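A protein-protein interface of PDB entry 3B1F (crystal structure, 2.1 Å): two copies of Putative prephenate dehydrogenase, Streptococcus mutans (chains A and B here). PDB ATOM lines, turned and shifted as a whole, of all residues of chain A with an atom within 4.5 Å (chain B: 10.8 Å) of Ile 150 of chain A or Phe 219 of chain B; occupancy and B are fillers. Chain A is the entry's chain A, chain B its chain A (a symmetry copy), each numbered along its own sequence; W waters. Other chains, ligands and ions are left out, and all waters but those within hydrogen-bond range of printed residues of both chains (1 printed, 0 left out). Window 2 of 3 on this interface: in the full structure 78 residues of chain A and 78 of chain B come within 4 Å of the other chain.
The backbone NH (N) of Ile 150 of chain A lies within hydrogen-bond range of the backbone carbonyl oxygen (O) of His 126 of chain A. N of Met 128 of chain A is in hydrogen-bond range of O of Tyr 148 of chain A (2.9 Å). The backbone NH (N) of Ile 179 of chain A sits at hydrogen-bond distance from the backbone carbonyl oxygen (O) of Phe 151 of chain A. The backbone carbonyl oxygen of Ile 179 of chain A is in hydrogen-bond range of the side-chain hydroxyl of Ser 152 of chain A, 2.8 Å away. The backbone carbonyl oxygen of Phe 209 of chain B sits at hydrogen-bond distance from a ring nitrogen (ND1) of His 213 of chain B (3.4 Å). O of Ala 220 of chain B lies within hydrogen-bond range of NH2 of Arg 225 of chain B, 3.1 Å away.
His 218 of chain B touches Tyr 148 of chain A (O to CE2, 3.2 Å). Phe 219 of chain B touches Ile 150 of chain A (CZ to CG1, 3.8 Å). CG of Met 215 of chain B touches CD1 of Ile 179 of chain A, 3.9 Å away. CG2 of Val 187 of chain A touches CB of His 213 of chain B, at 3.9 Å. Thr 216 of chain B touches Val 187 of chain A (N to CG1, 3.6 Å). CG1 of Val 187 of chain A touches CD2 of Phe 219 of chain B (3.6 Å). Thr 216 of chain B touches Ile 191 of chain A (CG2 to CG2, 3.7 Å). Ile 191 of chain A touches Phe 219 of chain B (CD1 to O, 3.4 Å). CD1 of Ile 191 of chain A touches N of Ala 220 of chain B, 3.996 Å away. O of Ile 191 of chain A touches CB of Phe 224 of chain B, 3.5 Å away.
Ile 150 of chain A touches just one residue of chain B: Phe 219 (3.8 Å). Of the printed residues of chain A, Phe 219 of chain B touches Met 128 (3.8 Å), Tyr 148 (3.99 Å), Ile 150 (3.8 Å), Val 187 (3.6 Å) and Ile 191 (3.4 Å). No residue of chain B comes within 4 Å of Gly 124 of chain A. His 126 of chain A touches none of the printed residues of chain B. No residue of chain B comes within 4 Å of Tyr 149 of chain A. Of chain B, only Met 215 comes within 4 Å of Ile 179 of chain A. Of the printed residues of chain A, Phe 224 of chain B touches Ile 191. Of the printed residues of chain B, Ile 191 of chain A touches Thr 216 (3.7 Å), Phe 219 (3.4 Å), Ala 220 (3.996 Å) and Phe 224 (3.5 Å). Of the printed residues of chain B, Val 187 of chain A touches His 213 (3.9 Å), Met 215 (3.8 Å), Thr 216 (3.6 Å) and Phe 219 (3.6 Å). Printed residues of chain A within 4 Å of His 213 of chain B: Val 187. Of the printed residues of chain A, Ala 220 of chain B touches Ile 191. The nearest residue of chain B that does not touch Ile 150 of chain A is Met 215 of chain B (7.6 Å). The nearest printed residue of chain A that does not touch Phe 219 of chain B is Ile 179 of chain A (4.1 Å).
Hydrophobic or aromatic side chains of chain B within 4 Å of the printed part of chain A: His 213, Met 215, His 218, Phe 219 and Phe 224. Of the 15 printed residues of chain A, 6 touch a printed residue of chain B. Printed residues of chain A that touch a printed residue of chain B: Met 128, Tyr 148, Ile 150, Ile 179, Val 187 and Ile 191. Among the printed residues, no Asp or Glu carboxylate lies within 4 Å of a Lys or Arg side-chain nitrogen of the other chain.
No position is printed for both chains.
Water W1 lies within hydrogen-bond range of N of Ala 221 of chain B, O of Ile 191 of chain A and N of Phe 224 of chain B.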
ATOM      1  N   GLY A 124     -12.962  20.300  15.797  1.00  0.00           N
ATOM      2  CA  GLY A 124     -12.974  21.688  15.379  1.00  0.00           C
ATOM      3  C   GLY A 124     -14.290  21.995  14.673  1.00  0.00           C
ATOM      4  O   GLY A 124     -14.804  21.150  13.922  1.00  0.00           O
ATOM      5  N   SER A 125     -14.833  23.191  14.900  1.00  0.00           N
ATOM      6  CA  SER A 125     -16.033  23.673  14.178  1.00  0.00           C
ATOM      7  C   SER A 125     -15.764  25.055  13.610  1.00  0.00           C
ATOM      8  O   SER A 125     -14.999  25.831  14.172  1.00  0.00           O
ATOM      9  CB  SER A 125     -17.250  23.858  15.105  1.00  0.00           C
ATOM     10  OG  SER A 125     -17.853  22.679  15.580  1.00  0.00           O
ATOM     11  N   HIS A 126     -16.378  25.341  12.473  1.00  0.00           N
ATOM     12  CA  HIS A 126     -16.441  26.678  11.891  1.00  0.00           C
ATOM     13  C   HIS A 126     -17.835  26.837  11.289  1.00  0.00           C
ATOM     14  O   HIS A 126     -18.127  26.294  10.209  1.00  0.00           O
ATOM     15  CB  HIS A 126     -15.312  26.956  10.894  1.00  0.00           C
ATOM     16  CG  HIS A 126     -15.456  28.270  10.144  1.00  0.00           C
ATOM     17  ND1 HIS A 126     -14.805  28.513   8.946  1.00  0.00           N
ATOM     18  CD2 HIS A 126     -16.142  29.415  10.421  1.00  0.00           C
ATOM     19  CE1 HIS A 126     -15.086  29.740   8.517  1.00  0.00           C
ATOM     20  NE2 HIS A 126     -15.901  30.302   9.389  1.00  0.00           N
ATOM     21  N   MET A 128     -19.998  28.850   9.273  1.00  0.00           N
ATOM     22  CA  MET A 128     -19.686  30.011   8.400  1.00  0.00           C
ATOM     23  C   MET A 128     -20.912  30.922   8.353  1.00  0.00           C
ATOM     24  O   MET A 128     -21.896  30.562   7.743  1.00  0.00           O
ATOM     25  CB  MET A 128     -19.429  29.542   7.002  1.00  0.00           C
ATOM     26  CG  MET A 128     -18.247  28.776   6.891  1.00  0.00           C
ATOM     27  SD  MET A 128     -17.685  28.481   5.046  1.00  0.00           S
ATOM     28  CE  MET A 128     -15.817  28.050   5.435  1.00  0.00           C
ATOM     29  N   TYR A 148     -22.628  26.747   5.460  1.00  0.00           N
ATOM     30  CA  TYR A 148     -21.886  25.557   5.759  1.00  0.00           C
ATOM     31  C   TYR A 148     -21.438  25.619   7.233  1.00  0.00           C
ATOM     32  O   TYR A 148     -20.910  26.628   7.667  1.00  0.00           O
ATOM     33  CB  TYR A 148     -20.647  25.475   4.855  1.00  0.00           C
ATOM     34  CG  TYR A 148     -20.957  25.061   3.412  1.00  0.00           C
ATOM     35  CD1 TYR A 148     -21.241  23.718   3.087  1.00  0.00           C
ATOM     36  CD2 TYR A 148     -20.936  25.999   2.372  1.00  0.00           C
ATOM     37  CE1 TYR A 148     -21.532  23.338   1.786  1.00  0.00           C
ATOM     38  CE2 TYR A 148     -21.234  25.619   1.051  1.00  0.00           C
ATOM     39  CZ  TYR A 148     -21.506  24.304   0.780  1.00  0.00           C
ATOM     40  OH  TYR A 148     -21.803  23.916  -0.487  1.00  0.00           O
ATOM     41  N   TYR A 149     -21.626  24.506   7.950  1.00  0.00           N
ATOM     42  CA  TYR A 149     -21.082  24.331   9.261  1.00  0.00           C
ATOM     43  C   TYR A 149     -19.983  23.283   9.122  1.00  0.00           C
ATOM     44  O   TYR A 149     -20.248  22.088   8.789  1.00  0.00           O
ATOM     45  CB  TYR A 149     -22.187  23.868  10.225  1.00  0.00           C
ATOM     46  CG  TYR A 149     -21.697  23.786  11.667  1.00  0.00           C
ATOM     47  CD1 TYR A 149     -22.110  24.719  12.606  1.00  0.00           C
ATOM     48  CD2 TYR A 149     -20.747  22.822  12.051  1.00  0.00           C
ATOM     49  CE1 TYR A 149     -21.645  24.687  13.908  1.00  0.00           C
ATOM     50  CE2 TYR A 149     -20.264  22.779  13.342  1.00  0.00           C
ATOM     51  CZ  TYR A 149     -20.718  23.709  14.277  1.00  0.00           C
ATOM     52  OH  TYR A 149     -20.262  23.656  15.590  1.00  0.00           O
ATOM     53  N   ILE A 150     -18.744  23.710   9.377  1.00  0.00           N
ATOM     54  CA  ILE A 150     -17.624  22.870   9.051  1.00  0.00           C
ATOM     55  C   ILE A 150     -17.183  22.125  10.323  1.00  0.00           C
ATOM     56  O   ILE A 150     -17.065  22.752  11.416  1.00  0.00           O
ATOM     57  CB  ILE A 150     -16.440  23.727   8.562  1.00  0.00           C
ATOM     58  CG1 ILE A 150     -16.543  24.166   7.107  1.00  0.00           C
ATOM     59  CG2 ILE A 150     -15.209  22.983   8.638  1.00  0.00           C
ATOM     60  CD1 ILE A 150     -17.868  24.457   6.615  1.00  0.00           C
ATOM     61  N   PHE A 151     -16.919  20.818  10.187  1.00  0.00           N
ATOM     62  CA  PHE A 151     -16.192  20.054  11.197  1.00  0.00           C
ATOM     63  C   PHE A 151     -14.783  19.641  10.697  1.00  0.00           C
ATOM     64  O   PHE A 151     -14.612  19.208   9.579  1.00  0.00           O
ATOM     65  CB  PHE A 151     -16.921  18.767  11.588  1.00  0.00           C
ATOM     66  CG  PHE A 151     -18.314  18.958  12.120  1.00  0.00           C
ATOM     67  CD1 PHE A 151     -18.533  19.235  13.467  1.00  0.00           C
ATOM     68  CD2 PHE A 151     -19.421  18.804  11.277  1.00  0.00           C
ATOM     69  CE1 PHE A 151     -19.840  19.387  13.974  1.00  0.00           C
ATOM     70  CE2 PHE A 151     -20.707  18.978  11.776  1.00  0.00           C
ATOM     71  CZ  PHE A 151     -20.908  19.277  13.129  1.00  0.00           C
ATOM     72  N   SER A 152     -13.780  19.794  11.551  1.00  0.00           N
ATOM     73  CA  SER A 152     -12.424  19.374  11.236  1.00  0.00           C
ATOM     74  C   SER A 152     -11.990  18.385  12.322  1.00  0.00           C
ATOM     75  O   SER A 152     -11.810  18.800  13.488  1.00  0.00           O
ATOM     76  CB  SER A 152     -11.421  20.564  11.153  1.00  0.00           C
ATOM     77  OG  SER A 152     -11.686  21.417  10.036  1.00  0.00           O
ATOM     78  N   VAL A 177     -20.349  19.859   6.779  1.00  0.00           N
ATOM     79  CA  VAL A 177     -19.252  19.452   5.910  1.00  0.00           C
ATOM     80  C   VAL A 177     -18.096  19.063   6.807  1.00  0.00           C
ATOM     81  O   VAL A 177     -17.752  19.803   7.709  1.00  0.00           O
ATOM     82  CB  VAL A 177     -18.759  20.656   5.000  1.00  0.00           C
ATOM     83  CG1 VAL A 177     -17.605  20.212   4.124  1.00  0.00           C
ATOM     84  CG2 VAL A 177     -19.872  21.116   4.087  1.00  0.00           C
ATOM     85  N   ILE A 179     -14.086  18.495   6.811  1.00  0.00           N
ATOM     86  CA  ILE A 179     -12.879  18.783   6.022  1.00  0.00           C
ATOM     87  C   ILE A 179     -11.642  18.884   6.943  1.00  0.00           C
ATOM     88  O   ILE A 179     -11.708  19.422   8.062  1.00  0.00           O
ATOM     89  CB  ILE A 179     -13.076  20.104   5.203  1.00  0.00           C
ATOM     90  CG1 ILE A 179     -11.839  20.455   4.333  1.00  0.00           C
ATOM     91  CG2 ILE A 179     -13.435  21.259   6.137  1.00  0.00           C
ATOM     92  CD1 ILE A 179     -12.115  21.645   3.436  1.00  0.00           C
ATOM     93  N   HIS A 184      -9.014  23.145   5.016  1.00  0.00           N
ATOM     94  CA  HIS A 184      -9.915  24.271   5.328  1.00  0.00           C
ATOM     95  C   HIS A 184      -9.208  25.633   5.342  1.00  0.00           C
ATOM     96  O   HIS A 184      -9.724  26.651   4.809  1.00  0.00           O
ATOM     97  CB  HIS A 184     -10.571  24.054   6.732  1.00  0.00           C
ATOM     98  CG  HIS A 184     -11.333  25.245   7.215  1.00  0.00           C
ATOM     99  ND1 HIS A 184     -10.717  26.348   7.777  1.00  0.00           N
ATOM    100  CD2 HIS A 184     -12.665  25.530   7.183  1.00  0.00           C
ATOM    101  CE1 HIS A 184     -11.641  27.246   8.094  1.00  0.00           C
ATOM    102  NE2 HIS A 184     -12.830  26.776   7.730  1.00  0.00           N
ATOM    103  N   VAL A 187      -8.224  26.721   1.850  1.00  0.00           N
ATOM    104  CA  VAL A 187      -9.322  27.131   1.004  1.00  0.00           C
ATOM    105  C   VAL A 187      -9.851  28.522   1.388  1.00  0.00           C
ATOM    106  O   VAL A 187     -10.127  29.397   0.520  1.00  0.00           O
ATOM    107  CB  VAL A 187     -10.433  26.031   0.943  1.00  0.00           C
ATOM    108  CG1 VAL A 187     -11.757  26.557   0.304  1.00  0.00           C
ATOM    109  CG2 VAL A 187      -9.862  24.757   0.216  1.00  0.00           C
ATOM    110  N   THR A 188     -10.007  28.716   2.683  1.00  0.00           N
ATOM    111  CA  THR A 188     -10.570  29.950   3.185  1.00  0.00           C
ATOM    112  C   THR A 188      -9.577  31.121   3.072  1.00  0.00           C
ATOM    113  O   THR A 188     -10.014  32.273   2.970  1.00  0.00           O
ATOM    114  CB  THR A 188     -11.080  29.855   4.682  1.00  0.00           C
ATOM    115  OG1 THR A 188     -10.065  29.309   5.545  1.00  0.00           O
ATOM    116  CG2 THR A 188     -12.353  29.002   4.785  1.00  0.00           C
ATOM    117  N   ILE A 191     -10.386  32.110  -0.743  1.00  0.00           N
ATOM    118  CA  ILE A 191     -11.632  32.785  -1.054  1.00  0.00           C
ATOM    119  C   ILE A 191     -12.147  33.735  -0.019  1.00  0.00           C
ATOM    120  O   ILE A 191     -13.199  34.357  -0.230  1.00  0.00           O
ATOM    121  CB  ILE A 191     -12.735  31.818  -1.472  1.00  0.00           C
ATOM    122  CG1 ILE A 191     -12.751  30.627  -0.561  1.00  0.00           C
ATOM    123  CG2 ILE A 191     -12.429  31.357  -2.968  1.00  0.00           C
ATOM    124  CD1 ILE A 191     -13.543  30.752   0.751  1.00  0.00           C
ATOM    125  N   ALA B 206      -8.074  32.247  -7.893  1.00  0.00           N
ATOM    126  CA  ALA B 206      -9.004  31.363  -7.172  1.00  0.00           C
ATOM    127  C   ALA B 206      -9.420  30.179  -8.119  1.00  0.00           C
ATOM    128  O   ALA B 206      -9.629  29.043  -7.685  1.00  0.00           O
ATOM    129  CB  ALA B 206     -10.261  32.135  -6.698  1.00  0.00           C
ATOM    130  N   PHE B 209      -6.555  27.680  -8.227  1.00  0.00           N
ATOM    131  CA  PHE B 209      -6.554  27.020  -6.936  1.00  0.00           C
ATOM    132  C   PHE B 209      -7.678  25.992  -6.823  1.00  0.00           C
ATOM    133  O   PHE B 209      -7.515  24.887  -6.327  1.00  0.00           O
ATOM    134  CB  PHE B 209      -6.732  28.166  -5.871  1.00  0.00           C
ATOM    135  CG  PHE B 209      -6.386  27.763  -4.463  1.00  0.00           C
ATOM    136  CD1 PHE B 209      -5.060  27.794  -4.012  1.00  0.00           C
ATOM    137  CD2 PHE B 209      -7.379  27.313  -3.592  1.00  0.00           C
ATOM    138  CE1 PHE B 209      -4.715  27.412  -2.749  1.00  0.00           C
ATOM    139  CE2 PHE B 209      -7.042  26.945  -2.287  1.00  0.00           C
ATOM    140  CZ  PHE B 209      -5.694  27.006  -1.883  1.00  0.00           C
ATOM    141  N   SER B 210      -8.854  26.392  -7.243  1.00  0.00           N
ATOM    142  CA  SER B 210     -10.029  25.555  -7.338  1.00  0.00           C
ATOM    143  C   SER B 210      -9.767  24.170  -7.929  1.00  0.00           C
ATOM    144  O   SER B 210     -10.265  23.171  -7.420  1.00  0.00           O
ATOM    145  CB  SER B 210     -11.010  26.245  -8.265  1.00  0.00           C
ATOM    146  OG  SER B 210     -12.262  25.736  -7.968  1.00  0.00           O
ATOM    147  N   HIS B 213      -8.246  22.194  -5.200  1.00  0.00           N
ATOM    148  CA  HIS B 213      -8.844  22.261  -3.845  1.00  0.00           C
ATOM    149  C   HIS B 213     -10.328  22.394  -4.006  1.00  0.00           C
ATOM    150  O   HIS B 213     -10.823  23.489  -4.238  1.00  0.00           O
ATOM    151  CB  HIS B 213      -8.343  23.490  -3.107  1.00  0.00           C
ATOM    152  CG  HIS B 213      -6.919  23.380  -2.709  1.00  0.00           C
ATOM    153  ND1 HIS B 213      -5.888  23.855  -3.487  1.00  0.00           N
ATOM    154  CD2 HIS B 213      -6.342  22.764  -1.666  1.00  0.00           C
ATOM    155  CE1 HIS B 213      -4.736  23.606  -2.893  1.00  0.00           C
ATOM    156  NE2 HIS B 213      -4.990  22.960  -1.773  1.00  0.00           N
ATOM    157  N   GLU B 214     -11.030  21.291  -3.900  1.00  0.00           N
ATOM    158  CA  GLU B 214     -12.401  21.262  -4.367  1.00  0.00           C
ATOM    159  C   GLU B 214     -13.384  22.130  -3.606  1.00  0.00           C
ATOM    160  O   GLU B 214     -14.356  22.588  -4.191  1.00  0.00           O
ATOM    161  CB  GLU B 214     -12.935  19.839  -4.461  1.00  0.00           C
ATOM    162  CG  GLU B 214     -12.984  19.184  -3.115  1.00  0.00           C
ATOM    163  CD  GLU B 214     -13.704  17.821  -3.079  1.00  0.00           C
ATOM    164  OE1 GLU B 214     -14.646  17.541  -3.874  1.00  0.00           O
ATOM    165  OE2 GLU B 214     -13.338  17.047  -2.174  1.00  0.00           O
ATOM    166  N   MET B 215     -13.163  22.357  -2.311  1.00  0.00           N
ATOM    167  CA  MET B 215     -14.156  23.145  -1.578  1.00  0.00           C
ATOM    168  C   MET B 215     -14.166  24.636  -1.926  1.00  0.00           C
ATOM    169  O   MET B 215     -15.100  25.303  -1.583  1.00  0.00           O
ATOM    170  CB  MET B 215     -14.098  22.883  -0.067  1.00  0.00           C
ATOM    171  CG  MET B 215     -14.422  21.452   0.313  1.00  0.00           C
ATOM    172  SD  MET B 215     -16.303  21.014  -0.137  1.00  0.00           S
ATOM    173  CE  MET B 215     -16.111  20.142  -1.883  1.00  0.00           C
ATOM    174  N   THR B 216     -13.155  25.118  -2.654  1.00  0.00           N
ATOM    175  CA  THR B 216     -13.067  26.495  -3.151  1.00  0.00           C
ATOM    176  C   THR B 216     -14.318  27.062  -3.807  1.00  0.00           C
ATOM    177  O   THR B 216     -14.742  28.227  -3.490  1.00  0.00           O
ATOM    178  CB  THR B 216     -11.870  26.666  -4.083  1.00  0.00           C
ATOM    179  OG1 THR B 216     -10.725  26.108  -3.457  1.00  0.00           O
ATOM    180  CG2 THR B 216     -11.565  28.138  -4.478  1.00  0.00           C
ATOM    181  N   LYS B 217     -14.916  26.276  -4.702  1.00  0.00           N
ATOM    182  CA  LYS B 217     -16.095  26.709  -5.437  1.00  0.00           C
ATOM    183  C   LYS B 217     -17.235  26.859  -4.427  1.00  0.00           C
ATOM    184  O   LYS B 217     -18.104  27.744  -4.550  1.00  0.00           O
ATOM    185  CB  LYS B 217     -16.584  25.594  -6.365  1.00  0.00           C
ATOM    186  CG  LYS B 217     -15.650  25.110  -7.519  1.00  0.00           C
ATOM    187  CD  LYS B 217     -16.330  23.888  -8.285  1.00  0.00           C
ATOM    188  CE  LYS B 217     -17.488  24.335  -9.245  1.00  0.00           C
ATOM    189  NZ  LYS B 217     -18.175  23.195  -9.986  1.00  0.00           N
ATOM    190  N   HIS B 218     -17.280  25.932  -3.478  1.00  0.00           N
ATOM    191  CA  HIS B 218     -18.415  25.898  -2.572  1.00  0.00           C
ATOM    192  C   HIS B 218     -18.348  26.933  -1.398  1.00  0.00           C
ATOM    193  O   HIS B 218     -19.397  27.372  -0.921  1.00  0.00           O
ATOM    194  CB  HIS B 218     -18.640  24.487  -2.053  1.00  0.00           C
ATOM    195  CG  HIS B 218     -18.711  23.460  -3.142  1.00  0.00           C
ATOM    196  ND1 HIS B 218     -19.836  23.275  -3.920  1.00  0.00           N
ATOM    197  CD2 HIS B 218     -17.775  22.601  -3.615  1.00  0.00           C
ATOM    198  CE1 HIS B 218     -19.602  22.312  -4.793  1.00  0.00           C
ATOM    199  NE2 HIS B 218     -18.359  21.888  -4.632  1.00  0.00           N
ATOM    200  N   PHE B 219     -17.145  27.315  -0.965  1.00  0.00           N
ATOM    201  CA  PHE B 219     -17.000  28.132   0.247  1.00  0.00           C
ATOM    202  C   PHE B 219     -16.945  29.578  -0.069  1.00  0.00           C
ATOM    203  O   PHE B 219     -16.941  30.388   0.867  1.00  0.00           O
ATOM    204  CB  PHE B 219     -15.714  27.813   1.028  1.00  0.00           C
ATOM    205  CG  PHE B 219     -15.773  26.546   1.857  1.00  0.00           C
ATOM    206  CD1 PHE B 219     -16.960  25.851   2.027  1.00  0.00           C
ATOM    207  CD2 PHE B 219     -14.618  26.078   2.473  1.00  0.00           C
ATOM    208  CE1 PHE B 219     -17.019  24.688   2.808  1.00  0.00           C
ATOM    209  CE2 PHE B 219     -14.624  24.918   3.245  1.00  0.00           C
ATOM    210  CZ  PHE B 219     -15.818  24.197   3.417  1.00  0.00           C
ATOM    211  N   ALA B 220     -16.839  29.930  -1.353  1.00  0.00           N
ATOM    212  CA  ALA B 220     -16.748  31.297  -1.778  1.00  0.00           C
ATOM    213  C   ALA B 220     -18.034  31.992  -1.343  1.00  0.00           C
ATOM    214  O   ALA B 220     -19.138  31.504  -1.666  1.00  0.00           O
ATOM    215  CB  ALA B 220     -16.577  31.385  -3.325  1.00  0.00           C
ATOM    216  N   ALA B 221     -17.941  33.143  -0.641  1.00  0.00           N
ATOM    217  CA  ALA B 221     -19.236  33.765  -0.238  1.00  0.00           C
ATOM    218  C   ALA B 221     -19.390  35.180  -0.802  1.00  0.00           C
ATOM    219  O   ALA B 221     -18.721  35.533  -1.781  1.00  0.00           O
ATOM    220  CB  ALA B 221     -19.459  33.680   1.327  1.00  0.00           C
ATOM    221  N   GLY B 222     -20.272  35.973  -0.225  1.00  0.00           N
ATOM    222  CA  GLY B 222     -20.543  37.339  -0.718  1.00  0.00           C
ATOM    223  C   GLY B 222     -19.302  38.193  -0.843  1.00  0.00           C
ATOM    224  O   GLY B 222     -19.174  38.989  -1.782  1.00  0.00           O
ATOM    225  N   GLY B 223     -18.350  38.026   0.062  1.00  0.00           N
ATOM    226  CA  GLY B 223     -17.081  38.763  -0.045  1.00  0.00           C
ATOM    227  C   GLY B 223     -16.446  38.532  -1.436  1.00  0.00           C
ATOM    228  O   GLY B 223     -16.111  39.484  -2.170  1.00  0.00           O
ATOM    229  N   PHE B 224     -16.330  37.267  -1.809  1.00  0.00           N
ATOM    230  CA  PHE B 224     -15.540  36.915  -2.945  1.00  0.00           C
ATOM    231  C   PHE B 224     -16.330  37.257  -4.211  1.00  0.00           C
ATOM    232  O   PHE B 224     -15.772  37.762  -5.152  1.00  0.00           O
ATOM    233  CB  PHE B 224     -15.189  35.433  -2.893  1.00  0.00           C
ATOM    234  CG  PHE B 224     -14.369  35.018  -4.036  1.00  0.00           C
ATOM    235  CD1 PHE B 224     -13.003  35.248  -4.039  1.00  0.00           C
ATOM    236  CD2 PHE B 224     -14.976  34.469  -5.177  1.00  0.00           C
ATOM    237  CE1 PHE B 224     -12.223  34.875  -5.165  1.00  0.00           C
ATOM    238  CE2 PHE B 224     -14.196  34.080  -6.287  1.00  0.00           C
ATOM    239  CZ  PHE B 224     -12.820  34.306  -6.275  1.00  0.00           C
ATOM    240  N   ARG B 225     -17.620  36.935  -4.225  1.00  0.00           N
ATOM    241  CA  ARG B 225     -18.524  37.302  -5.325  1.00  0.00           C
ATOM    242  C   ARG B 225     -18.470  38.762  -5.702  1.00  0.00           C
ATOM    243  O   ARG B 225     -18.514  39.066  -6.915  1.00  0.00           O
ATOM    244  CB  ARG B 225     -19.944  36.970  -4.983  1.00  0.00           C
ATOM    245  CG  ARG B 225     -20.364  35.548  -5.376  1.00  0.00           C
ATOM    246  CD  ARG B 225     -21.808  35.200  -4.847  1.00  0.00           C
ATOM    247  NE  ARG B 225     -21.934  33.777  -4.466  1.00  0.00           N
ATOM    248  CZ  ARG B 225     -21.802  33.288  -3.220  1.00  0.00           C
ATOM    249  NH1 ARG B 225     -21.526  34.092  -2.195  1.00  0.00           N
ATOM    250  NH2 ARG B 225     -21.949  31.976  -2.973  1.00  0.00           N
HETATM  251  O   HOH W   1     -16.041  34.938   0.687  1.00  0.00           O
